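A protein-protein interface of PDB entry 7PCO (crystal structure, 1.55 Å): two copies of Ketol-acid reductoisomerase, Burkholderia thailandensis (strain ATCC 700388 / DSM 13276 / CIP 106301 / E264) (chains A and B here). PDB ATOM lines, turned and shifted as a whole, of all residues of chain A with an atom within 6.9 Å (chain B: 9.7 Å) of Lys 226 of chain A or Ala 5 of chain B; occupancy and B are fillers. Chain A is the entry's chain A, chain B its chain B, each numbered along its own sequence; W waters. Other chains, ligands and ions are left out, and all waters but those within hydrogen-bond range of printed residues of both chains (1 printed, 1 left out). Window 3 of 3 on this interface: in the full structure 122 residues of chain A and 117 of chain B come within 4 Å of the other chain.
Leu 195 of chain B touches Phe 223 of chain A (N to CE2, 3.8 Å).
OD1 of Asn 224 of chain A touches CE of Met 185 of chain B, at 3.6 Å.
Asn 224 of chain A touches Leu 187 of chain B (CB to CD1, 3.8 Å).
CD of Lys 226 of chain A touches CD1 of Ile 10 of chain B, at 3.98 Å.
Met 185 of chain B touches Ala 227 of chain A (CE to CB, 3.95 Å).
Leu 195 of chain B touches Ala 227 of chain A (CD2 to CB, 3.5 Å).
OH of Tyr 155 of chain B touches CB of Leu 230 of chain A, 3.5 Å away.
Leu 195 of chain B touches Glu 231 of chain A (CG to CG, 3.5 Å).
Phe 332 of chain A touches Ile 10 of chain B.
Phe 332 of chain A touches Met 185 of chain B (CZ to CB, 3.9 Å).
No residue of chain B comes within 4 Å of Pro 225 of chain A.
Printed residues of chain B within 4 Å of Lys 226 of chain A: Ala 5, Asp 8 and Ile 10.
Of chain B, only Tyr 155 (3.3 Å), Met 185 (3.95 Å) and Leu 195 (3.5 Å) come within 4 Å of Ala 227 of chain A.
Of chain A, only Lys 226 comes within 4 Å of Ala 5 of chain B.
Printed residues of chain A within 4 Å of Ile 10 of chain B: Lys 226, Ala 331 and Phe 332.
Printed residues of chain A within 4 Å of Gln 191 of chain B: Phe 223 (3.4 Å) and Asn 224 (2.8 Å).
The nearest printed residue of chain B that does not touch Lys 226 of chain A is Met 185 of chain B (4.2 Å).
The nearest residue of chain A that does not touch Ala 5 of chain B is Gln 327 of chain A (4.3 Å).
The guanidinium group (NE) of Arg 136 of chain B lies within salt-bridge range of the side-chain carboxylate (OE2) of Glu 231 of chain A (2.8 Å).
The side-chain hydroxyl (OH) of Tyr 155 of chain B lies close to the backbone carbonyl oxygen (O) of Ala 227 of chain A (3.3 Å).
The side-chain carboxylate (OD1) of Asp 8 of chain B is in hydrogen-bond range of the side-chain amide nitrogen (ND2) of Asn 224 of chain A (2.8 Å).
The side-chain amino group (NZ) of Lys 226 of chain A is in salt-bridge range of the side-chain carboxylate (OD2) of Asp 8 of chain B (2.8 Å).
N of Asn 224 of chain A sits at hydrogen-bond distance from OE1 of Gln 191 of chain B (2.8 Å).
The side-chain carboxylate (OE2) of Glu 231 of chain A is in hydrogen-bond range of the side-chain hydroxyl (OH) of Tyr 155 of chain B.
The side-chain amino group (NZ) of Lys 226 of chain A lies within hydrogen-bond range of the backbone carbonyl oxygen (O) of Ala 5 of chain B.
Of the 17 printed residues of chain B, 9 touch a printed residue of chain A.
Hydrophobic or aromatic side chains of chain B within 4 Å of the printed part of chain A: Ala 5, Ile 10, Tyr 155, Met 185, Leu 187 and Leu 195.
Printed residues of chain A that touch a printed residue of chain B: Phe 223, Asn 224, Lys 226, Ala 227, Leu 230, Glu 231, Ala 331 and Phe 332.
Hydrophobic or aromatic side chains of chain A within 4 Å of the printed part of chain B: Phe 223, Ala 227, Leu 230, Ala 331 and Phe 332.
N of Arg 136 of chain B lies within hydrogen-bond range of O of Pro 153 of chain B, at 3.0 Å.
The backbone carbonyl oxygen (O) of Ala 154 of chain B is in hydrogen-bond range of the backbone NH (N) of Met 185 of chain B (3.0 Å).
The side-chain amide oxygen of Asn 224 of chain A is in hydrogen-bond range of the backbone NH of Lys 226 of chain A, 3.0 Å away.
The backbone NH (N) of Ala 227 of chain A is in hydrogen-bond range of the side-chain amide oxygen (OD1) of Asn 224 of chain A, at 3.1 Å.
Water W1 lies within hydrogen-bond range of the backbone carbonyl oxygen (O) of Arg 136 of chain B (2.8 Å) and the side-chain carboxylate (OE1) of Glu 231 of chain A (2.9 Å).
No position is printed for both chains.
Of the 19 pairs that touch across the chains among the printed residues, none has its exchanged pair printed and touching as well.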
ATOM      1  N   PHE A 215     -29.105  -7.287 -17.661  1.00  0.00           N
ATOM      2  CA  PHE A 215     -28.449  -5.962 -17.539  1.00  0.00           C
ATOM      3  C   PHE A 215     -27.444  -5.991 -16.384  1.00  0.00           C
ATOM      4  O   PHE A 215     -26.277  -5.582 -16.596  1.00  0.00           O
ATOM      5  CB  PHE A 215     -29.480  -4.857 -17.318  1.00  0.00           C
ATOM      6  CG  PHE A 215     -28.868  -3.514 -17.008  1.00  0.00           C
ATOM      7  CD1 PHE A 215     -28.288  -2.763 -18.017  1.00  0.00           C
ATOM      8  CD2 PHE A 215     -28.884  -2.999 -15.718  1.00  0.00           C
ATOM      9  CE1 PHE A 215     -27.728  -1.526 -17.739  1.00  0.00           C
ATOM     10  CE2 PHE A 215     -28.326  -1.756 -15.444  1.00  0.00           C
ATOM     11  CZ  PHE A 215     -27.768  -1.017 -16.459  1.00  0.00           C
ATOM     12  N   VAL A 219     -23.339  -5.696 -16.633  1.00  0.00           N
ATOM     13  CA  VAL A 219     -22.655  -4.533 -16.004  1.00  0.00           C
ATOM     14  C   VAL A 219     -21.614  -5.065 -15.010  1.00  0.00           C
ATOM     15  O   VAL A 219     -20.484  -4.534 -15.009  1.00  0.00           O
ATOM     16  CB  VAL A 219     -23.646  -3.539 -15.378  1.00  0.00           C
ATOM     17  CG1 VAL A 219     -22.915  -2.575 -14.457  1.00  0.00           C
ATOM     18  CG2 VAL A 219     -24.414  -2.790 -16.466  1.00  0.00           C
ATOM     19  N   PHE A 223     -19.265  -4.818 -18.958  1.00  0.00           N
ATOM     20  CA  PHE A 223     -19.827  -4.337 -20.242  1.00  0.00           C
ATOM     21  C   PHE A 223     -20.318  -2.895 -20.079  1.00  0.00           C
ATOM     22  O   PHE A 223     -20.746  -2.481 -18.974  1.00  0.00           O
ATOM     23  CB  PHE A 223     -20.935  -5.266 -20.763  1.00  0.00           C
ATOM     24  CG  PHE A 223     -20.418  -6.594 -21.246  1.00  0.00           C
ATOM     25  CD1 PHE A 223     -20.123  -7.605 -20.340  1.00  0.00           C
ATOM     26  CD2 PHE A 223     -20.190  -6.825 -22.594  1.00  0.00           C
ATOM     27  CE1 PHE A 223     -19.611  -8.817 -20.773  1.00  0.00           C
ATOM     28  CE2 PHE A 223     -19.692  -8.045 -23.023  1.00  0.00           C
ATOM     29  CZ  PHE A 223     -19.401  -9.036 -22.113  1.00  0.00           C
ATOM     30  N   ASN A 224     -20.249  -2.154 -21.184  1.00  0.00           N
ATOM     31  CA  ASN A 224     -20.807  -0.788 -21.341  1.00  0.00           C
ATOM     32  C   ASN A 224     -22.280  -0.785 -20.919  1.00  0.00           C
ATOM     33  O   ASN A 224     -23.093  -1.487 -21.509  1.00  0.00           O
ATOM     34  CB  ASN A 224     -20.610  -0.336 -22.786  1.00  0.00           C
ATOM     35  CG  ASN A 224     -21.028   1.096 -23.021  1.00  0.00           C
ATOM     36  OD1 ASN A 224     -22.215   1.400 -23.004  1.00  0.00           O
ATOM     37  ND2 ASN A 224     -20.058   1.973 -23.228  1.00  0.00           N
ATOM     38  N   PRO A 225     -22.693  -0.039 -19.863  1.00  0.00           N
ATOM     39  CA  PRO A 225     -24.105  -0.022 -19.462  1.00  0.00           C
ATOM     40  C   PRO A 225     -25.121   0.431 -20.528  1.00  0.00           C
ATOM     41  O   PRO A 225     -26.211  -0.119 -20.554  1.00  0.00           O
ATOM     42  CB  PRO A 225     -24.105   0.919 -18.247  1.00  0.00           C
ATOM     43  CG  PRO A 225     -22.719   0.733 -17.672  1.00  0.00           C
ATOM     44  CD  PRO A 225     -21.833   0.670 -18.900  1.00  0.00           C
ATOM     45  N   LYS A 226     -24.790   1.394 -21.387  1.00  0.00           N
ATOM     46  CA  LYS A 226     -25.727   1.770 -22.479  1.00  0.00           C
ATOM     47  C   LYS A 226     -25.921   0.563 -23.410  1.00  0.00           C
ATOM     48  O   LYS A 226     -27.071   0.287 -23.793  1.00  0.00           O
ATOM     49  CB  LYS A 226     -25.250   2.990 -23.262  1.00  0.00           C
ATOM     50  CG  LYS A 226     -25.356   4.319 -22.529  1.00  0.00           C
ATOM     51  CD  LYS A 226     -25.065   5.471 -23.468  1.00  0.00           C
ATOM     52  CE  LYS A 226     -25.209   6.822 -22.814  1.00  0.00           C
ATOM     53  NZ  LYS A 226     -24.099   7.091 -21.870  1.00  0.00           N
ATOM     54  N   ALA A 227     -24.839  -0.115 -23.787  1.00  0.00           N
ATOM     55  CA  ALA A 227     -24.909  -1.285 -24.692  1.00  0.00           C
ATOM     56  C   ALA A 227     -25.698  -2.411 -24.013  1.00  0.00           C
ATOM     57  O   ALA A 227     -26.554  -3.042 -24.667  1.00  0.00           O
ATOM     58  CB  ALA A 227     -23.522  -1.727 -25.084  1.00  0.00           C
ATOM     59  N   ALA A 228     -25.411  -2.681 -22.741  1.00  0.00           N
ATOM     60  CA  ALA A 228     -26.102  -3.744 -21.986  1.00  0.00           C
ATOM     61  C   ALA A 228     -27.612  -3.453 -21.997  1.00  0.00           C
ATOM     62  O   ALA A 228     -28.392  -4.384 -22.264  1.00  0.00           O
ATOM     63  CB  ALA A 228     -25.540  -3.856 -20.593  1.00  0.00           C
ATOM     64  N   LEU A 229     -27.998  -2.202 -21.738  1.00  0.00           N
ATOM     65  CA  LEU A 229     -29.421  -1.777 -21.665  1.00  0.00           C
ATOM     66  C   LEU A 229     -30.045  -1.920 -23.060  1.00  0.00           C
ATOM     67  O   LEU A 229     -31.153  -2.482 -23.162  1.00  0.00           O
ATOM     68  CB  LEU A 229     -29.472  -0.337 -21.137  1.00  0.00           C
ATOM     69  CG  LEU A 229     -30.823   0.242 -20.708  1.00  0.00           C
ATOM     70  CD1 LEU A 229     -31.794   0.409 -21.866  1.00  0.00           C
ATOM     71  CD2 LEU A 229     -31.446  -0.544 -19.571  1.00  0.00           C
ATOM     72  N   LEU A 230     -29.342  -1.500 -24.114  1.00  0.00           N
ATOM     73  CA  LEU A 230     -29.861  -1.636 -25.498  1.00  0.00           C
ATOM     74  C   LEU A 230     -30.116  -3.114 -25.823  1.00  0.00           C
ATOM     75  O   LEU A 230     -31.208  -3.424 -26.352  1.00  0.00           O
ATOM     76  CB  LEU A 230     -28.890  -1.016 -26.506  1.00  0.00           C
ATOM     77  CG  LEU A 230     -28.967   0.505 -26.618  1.00  0.00           C
ATOM     78  CD1 LEU A 230     -27.778   1.040 -27.395  1.00  0.00           C
ATOM     79  CD2 LEU A 230     -30.260   0.948 -27.275  1.00  0.00           C
ATOM     80  N   GLU A 231     -29.174  -4.005 -25.526  1.00  0.00           N
ATOM     81  CA  GLU A 231     -29.328  -5.430 -25.918  1.00  0.00           C
ATOM     82  C   GLU A 231     -30.460  -6.092 -25.130  1.00  0.00           C
ATOM     83  O   GLU A 231     -31.199  -6.855 -25.744  1.00  0.00           O
ATOM     84  CB  GLU A 231     -28.010  -6.180 -25.762  1.00  0.00           C
ATOM     85  CG  GLU A 231     -26.935  -5.576 -26.631  1.00  0.00           C
ATOM     86  CD  GLU A 231     -27.419  -5.298 -28.037  1.00  0.00           C
ATOM     87  OE1 GLU A 231     -27.901  -6.251 -28.687  1.00  0.00           O
ATOM     88  OE2 GLU A 231     -27.349  -4.140 -28.468  1.00  0.00           O
ATOM     89  N   GLY A 234     -33.608  -2.174 -24.737  1.00  0.00           N
ATOM     90  CA  GLY A 234     -33.723  -0.765 -25.163  1.00  0.00           C
ATOM     91  C   GLY A 234     -33.556  -0.540 -26.662  1.00  0.00           C
ATOM     92  O   GLY A 234     -34.030   0.505 -27.162  1.00  0.00           O
ATOM     93  N   ALA A 324     -30.315   3.889 -16.201  1.00  0.00           N
ATOM     94  CA  ALA A 324     -29.666   3.574 -17.497  1.00  0.00           C
ATOM     95  C   ALA A 324     -30.669   3.822 -18.633  1.00  0.00           C
ATOM     96  O   ALA A 324     -30.254   4.329 -19.660  1.00  0.00           O
ATOM     97  CB  ALA A 324     -29.157   2.158 -17.498  1.00  0.00           C
ATOM     98  N   GLN A 327     -30.698   7.509 -19.548  1.00  0.00           N
ATOM     99  CA  GLN A 327     -29.426   7.874 -20.239  1.00  0.00           C
ATOM    100  C   GLN A 327     -29.470   7.384 -21.691  1.00  0.00           C
ATOM    101  O   GLN A 327     -29.122   8.157 -22.604  1.00  0.00           O
ATOM    102  CB  GLN A 327     -28.213   7.296 -19.513  1.00  0.00           C
ATOM    103  CG  GLN A 327     -28.022   7.900 -18.131  1.00  0.00           C
ATOM    104  CD  GLN A 327     -27.004   7.172 -17.292  1.00  0.00           C
ATOM    105  OE1 GLN A 327     -26.556   6.075 -17.624  1.00  0.00           O
ATOM    106  NE2 GLN A 327     -26.641   7.783 -16.176  1.00  0.00           N
ATOM    107  N   VAL A 328     -29.902   6.145 -21.918  1.00  0.00           N
ATOM    108  CA  VAL A 328     -29.949   5.568 -23.291  1.00  0.00           C
ATOM    109  C   VAL A 328     -30.971   6.328 -24.135  1.00  0.00           C
ATOM    110  O   VAL A 328     -30.654   6.672 -25.293  1.00  0.00           O
ATOM    111  CB  VAL A 328     -30.264   4.068 -23.235  1.00  0.00           C
ATOM    112  CG1 VAL A 328     -30.714   3.523 -24.580  1.00  0.00           C
ATOM    113  CG2 VAL A 328     -29.074   3.306 -22.684  1.00  0.00           C
ATOM    114  N   ALA A 331     -29.873   9.552 -25.479  1.00  0.00           N
ATOM    115  CA  ALA A 331     -28.694   9.381 -26.369  1.00  0.00           C
ATOM    116  C   ALA A 331     -29.065   8.747 -27.720  1.00  0.00           C
ATOM    117  O   ALA A 331     -28.327   8.957 -28.708  1.00  0.00           O
ATOM    118  CB  ALA A 331     -27.675   8.542 -25.652  1.00  0.00           C
ATOM    119  N   PHE A 332     -30.143   7.961 -27.750  1.00  0.00           N
ATOM    120  CA  PHE A 332     -30.615   7.184 -28.920  1.00  0.00           C
ATOM    121  C   PHE A 332     -32.076   7.517 -29.195  1.00  0.00           C
ATOM    122  O   PHE A 332     -32.921   7.401 -28.292  1.00  0.00           O
ATOM    123  CB  PHE A 332     -30.462   5.688 -28.661  1.00  0.00           C
ATOM    124  CG  PHE A 332     -29.033   5.214 -28.550  1.00  0.00           C
ATOM    125  CD1 PHE A 332     -28.392   5.186 -27.324  1.00  0.00           C
ATOM    126  CD2 PHE A 332     -28.340   4.770 -29.664  1.00  0.00           C
ATOM    127  CE1 PHE A 332     -27.091   4.729 -27.213  1.00  0.00           C
ATOM    128  CE2 PHE A 332     -27.034   4.321 -29.553  1.00  0.00           C
ATOM    129  CZ  PHE A 332     -26.418   4.280 -28.327  1.00  0.00           C
ATOM    130  N   MET B   4     -17.363   5.651 -17.633  1.00  0.00           N
ATOM    131  CA  MET B   4     -18.344   6.729 -17.263  1.00  0.00           C
ATOM    132  C   MET B   4     -19.209   7.029 -18.492  1.00  0.00           C
ATOM    133  O   MET B   4     -18.680   6.924 -19.610  1.00  0.00           O
ATOM    134  CB  MET B   4     -17.651   8.024 -16.813  1.00  0.00           C
ATOM    135  CG  MET B   4     -16.669   7.863 -15.657  1.00  0.00           C
ATOM    136  SD  MET B   4     -17.443   7.540 -14.048  1.00  0.00           S
ATOM    137  CE  MET B   4     -18.225   9.118 -13.702  1.00  0.00           C
ATOM    138  N   ALA B   5     -20.477   7.397 -18.279  1.00  0.00           N
ATOM    139  CA  ALA B   5     -21.505   7.615 -19.326  1.00  0.00           C
ATOM    140  C   ALA B   5     -21.062   8.720 -20.296  1.00  0.00           C
ATOM    141  O   ALA B   5     -21.363   8.602 -21.501  1.00  0.00           O
ATOM    142  CB  ALA B   5     -22.825   7.936 -18.670  1.00  0.00           C
ATOM    143  N   SER B   6     -20.354   9.741 -19.795  1.00  0.00           N
ATOM    144  CA  SER B   6     -19.833  10.897 -20.577  1.00  0.00           C
ATOM    145  C   SER B   6     -18.851  10.432 -21.663  1.00  0.00           C
ATOM    146  O   SER B   6     -18.744  11.141 -22.678  1.00  0.00           O
ATOM    147  CB  SER B   6     -19.199  11.922 -19.671  1.00  0.00           C
ATOM    148  OG  SER B   6     -18.225  11.321 -18.828  1.00  0.00           O
ATOM    149  N   ASN B   7     -18.171   9.292 -21.458  1.00  0.00           N
ATOM    150  CA  ASN B   7     -17.120   8.725 -22.354  1.00  0.00           C
ATOM    151  C   ASN B   7     -17.727   8.111 -23.629  1.00  0.00           C
ATOM    152  O   ASN B   7     -16.963   7.853 -24.579  1.00  0.00           O
ATOM    153  CB  ASN B   7     -16.293   7.654 -21.629  1.00  0.00           C
ATOM    154  CG  ASN B   7     -14.909   7.419 -22.204  1.00  0.00           C
ATOM    155  OD1 ASN B   7     -14.000   7.010 -21.484  1.00  0.00           O
ATOM    156  ND2 ASN B   7     -14.729   7.665 -23.492  1.00  0.00           N
ATOM    157  N   ASP B   8     -19.031   7.833 -23.665  1.00  0.00           N
ATOM    158  CA  ASP B   8     -19.661   7.158 -24.831  1.00  0.00           C
ATOM    159  C   ASP B   8     -19.676   8.112 -26.024  1.00  0.00           C
ATOM    160  O   ASP B   8     -20.037   9.295 -25.859  1.00  0.00           O
ATOM    161  CB  ASP B   8     -21.051   6.623 -24.482  1.00  0.00           C
ATOM    162  CG  ASP B   8     -20.980   5.521 -23.443  1.00  0.00           C
ATOM    163  OD1 ASP B   8     -20.035   4.727 -23.524  1.00  0.00           O
ATOM    164  OD2 ASP B   8     -21.862   5.473 -22.550  1.00  0.00           O
ATOM    165  N   LEU B   9     -19.264   7.601 -27.179  1.00  0.00           N
ATOM    166  CA  LEU B   9     -19.207   8.340 -28.461  1.00  0.00           C
ATOM    167  C   LEU B   9     -20.370   7.874 -29.339  1.00  0.00           C
ATOM    168  O   LEU B   9     -20.300   6.745 -29.860  1.00  0.00           O
ATOM    169  CB  LEU B   9     -17.860   8.036 -29.116  1.00  0.00           C
ATOM    170  CG  LEU B   9     -17.277   9.151 -29.969  1.00  0.00           C
ATOM    171  CD1 LEU B   9     -16.838  10.319 -29.093  1.00  0.00           C
ATOM    172  CD2 LEU B   9     -16.116   8.619 -30.792  1.00  0.00           C
ATOM    173  N   ILE B  10     -21.394   8.712 -29.493  1.00  0.00           N
ATOM    174  CA  ILE B  10     -22.653   8.336 -30.195  1.00  0.00           C
ATOM    175  C   ILE B  10     -22.895   9.344 -31.314  1.00  0.00           C
ATOM    176  O   ILE B  10     -23.021  10.549 -31.033  1.00  0.00           O
ATOM    177  CB  ILE B  10     -23.838   8.254 -29.219  1.00  0.00           C
ATOM    178  CG1 ILE B  10     -23.556   7.254 -28.092  1.00  0.00           C
ATOM    179  CG2 ILE B  10     -25.118   7.926 -29.968  1.00  0.00           C
ATOM    180  CD1 ILE B  10     -24.498   7.368 -26.926  1.00  0.00           C
ATOM    181  N   ARG B 136     -28.297  -3.339 -34.284  1.00  0.00           N
ATOM    182  CA  ARG B 136     -28.877  -3.909 -33.042  1.00  0.00           C
ATOM    183  C   ARG B 136     -30.300  -4.388 -33.322  1.00  0.00           C
ATOM    184  O   ARG B 136     -31.062  -4.545 -32.373  1.00  0.00           O
ATOM    185  CB  ARG B 136     -28.868  -2.887 -31.907  1.00  0.00           C
ATOM    186  CG  ARG B 136     -27.516  -2.241 -31.641  1.00  0.00           C
ATOM    187  CD  ARG B 136     -26.326  -3.154 -31.872  1.00  0.00           C
ATOM    188  NE  ARG B 136     -26.304  -4.386 -31.096  1.00  0.00           N
ATOM    189  CZ  ARG B 136     -25.441  -5.382 -31.294  1.00  0.00           C
ATOM    190  NH1 ARG B 136     -24.530  -5.284 -32.246  1.00  0.00           N
ATOM    191  NH2 ARG B 136     -25.473  -6.461 -30.526  1.00  0.00           N
ATOM    192  N   PRO B 153     -30.485   1.367 -33.762  1.00  0.00           N
ATOM    193  CA  PRO B 153     -29.126   1.654 -33.311  1.00  0.00           C
ATOM    194  C   PRO B 153     -28.120   0.707 -33.966  1.00  0.00           C
ATOM    195  O   PRO B 153     -28.509  -0.322 -34.453  1.00  0.00           O
ATOM    196  CB  PRO B 153     -29.138   1.352 -31.802  1.00  0.00           C
ATOM    197  CG  PRO B 153     -30.619   1.302 -31.427  1.00  0.00           C
ATOM    198  CD  PRO B 153     -31.323   0.835 -32.678  1.00  0.00           C
ATOM    199  N   ALA B 154     -26.844   1.065 -33.907  1.00  0.00           N
ATOM    200  CA  ALA B 154     -25.726   0.203 -34.342  1.00  0.00           C
ATOM    201  C   ALA B 154     -24.501   0.521 -33.477  1.00  0.00           C
ATOM    202  O   ALA B 154     -24.454   1.627 -32.897  1.00  0.00           O
ATOM    203  CB  ALA B 154     -25.478   0.426 -35.811  1.00  0.00           C
ATOM    204  N   TYR B 155     -23.584  -0.437 -33.343  1.00  0.00           N
ATOM    205  CA  TYR B 155     -22.227  -0.213 -32.779  1.00  0.00           C
ATOM    206  C   TYR B 155     -21.230  -0.186 -33.933  1.00  0.00           C
ATOM    207  O   TYR B 155     -21.456  -0.849 -34.966  1.00  0.00           O
ATOM    208  CB  TYR B 155     -21.857  -1.285 -31.754  1.00  0.00           C
ATOM    209  CG  TYR B 155     -22.895  -1.484 -30.679  1.00  0.00           C
ATOM    210  CD1 TYR B 155     -23.611  -0.417 -30.169  1.00  0.00           C
ATOM    211  CD2 TYR B 155     -23.170  -2.739 -30.169  1.00  0.00           C
ATOM    212  CE1 TYR B 155     -24.580  -0.594 -29.193  1.00  0.00           C
ATOM    213  CE2 TYR B 155     -24.125  -2.934 -29.185  1.00  0.00           C
ATOM    214  CZ  TYR B 155     -24.840  -1.860 -28.700  1.00  0.00           C
ATOM    215  OH  TYR B 155     -25.788  -2.050 -27.738  1.00  0.00           O
ATOM    216  N   VAL B 184     -25.354   5.717 -33.499  1.00  0.00           N
ATOM    217  CA  VAL B 184     -24.267   4.749 -33.788  1.00  0.00           C
ATOM    218  C   VAL B 184     -23.161   4.969 -32.764  1.00  0.00           C
ATOM    219  O   VAL B 184     -22.527   6.033 -32.784  1.00  0.00           O
ATOM    220  CB  VAL B 184     -23.805   4.886 -35.248  1.00  0.00           C
ATOM    221  CG1 VAL B 184     -22.611   4.006 -35.539  1.00  0.00           C
ATOM    222  CG2 VAL B 184     -24.941   4.552 -36.196  1.00  0.00           C
ATOM    223  N   MET B 185     -22.969   4.005 -31.868  1.00  0.00           N
ATOM    224  CA  MET B 185     -22.057   4.165 -30.711  1.00  0.00           C
ATOM    225  C   MET B 185     -20.770   3.393 -30.980  1.00  0.00           C
ATOM    226  O   MET B 185     -20.834   2.280 -31.485  1.00  0.00           O
ATOM    227  CB  MET B 185     -22.700   3.671 -29.414  1.00  0.00           C
ATOM    228  CG  MET B 185     -21.821   3.853 -28.205  1.00  0.00           C
ATOM    229  SD  MET B 185     -22.757   3.655 -26.679  1.00  0.00           S
ATOM    230  CE  MET B 185     -22.782   1.873 -26.535  1.00  0.00           C
ATOM    231  N   ALA B 186     -19.635   3.985 -30.634  1.00  0.00           N
ATOM    232  CA  ALA B 186     -18.325   3.306 -30.667  1.00  0.00           C
ATOM    233  C   ALA B 186     -18.322   2.200 -29.604  1.00  0.00           C
ATOM    234  O   ALA B 186     -18.617   2.478 -28.433  1.00  0.00           O
ATOM    235  CB  ALA B 186     -17.226   4.323 -30.446  1.00  0.00           C
ATOM    236  N   LEU B 187     -18.066   0.963 -30.005  1.00  0.00           N
ATOM    237  CA  LEU B 187     -17.926  -0.176 -29.065  1.00  0.00           C
ATOM    238  C   LEU B 187     -16.942  -1.144 -29.707  1.00  0.00           C
ATOM    239  O   LEU B 187     -17.074  -1.382 -30.906  1.00  0.00           O
ATOM    240  CB  LEU B 187     -19.294  -0.833 -28.829  1.00  0.00           C
ATOM    241  CG  LEU B 187     -19.323  -1.837 -27.677  1.00  0.00           C
ATOM    242  CD1 LEU B 187     -19.456  -1.123 -26.357  1.00  0.00           C
ATOM    243  CD2 LEU B 187     -20.445  -2.859 -27.832  1.00  0.00           C
ATOM    244  N   GLN B 191     -15.957  -6.764 -27.384  1.00  0.00           N
ATOM    245  CA  GLN B 191     -17.130  -6.503 -26.519  1.00  0.00           C
ATOM    246  C   GLN B 191     -18.424  -6.760 -27.307  1.00  0.00           C
ATOM    247  O   GLN B 191     -19.325  -7.407 -26.754  1.00  0.00           O
ATOM    248  CB  GLN B 191     -17.141  -5.085 -25.957  1.00  0.00           C
ATOM    249  CG  GLN B 191     -18.357  -4.889 -25.069  1.00  0.00           C
ATOM    250  CD  GLN B 191     -18.396  -3.658 -24.200  1.00  0.00           C
ATOM    251  OE1 GLN B 191     -19.373  -3.439 -23.483  1.00  0.00           O
ATOM    252  NE2 GLN B 191     -17.347  -2.855 -24.244  1.00  0.00           N
ATOM    253  N   LEU B 195     -21.285  -9.539 -26.144  1.00  0.00           N
ATOM    254  CA  LEU B 195     -22.570  -8.915 -25.742  1.00  0.00           C
ATOM    255  C   LEU B 195     -23.682  -9.474 -26.638  1.00  0.00           C
ATOM    256  O   LEU B 195     -24.711  -9.943 -26.119  1.00  0.00           O
ATOM    257  CB  LEU B 195     -22.425  -7.396 -25.867  1.00  0.00           C
ATOM    258  CG  LEU B 195     -23.711  -6.602 -25.688  1.00  0.00           C
ATOM    259  CD1 LEU B 195     -24.297  -6.843 -24.303  1.00  0.00           C
ATOM    260  CD2 LEU B 195     -23.454  -5.120 -25.926  1.00  0.00           C
HETATM  261  O   HOH W   1     -30.432  -5.475 -29.814  1.00  0.00           O
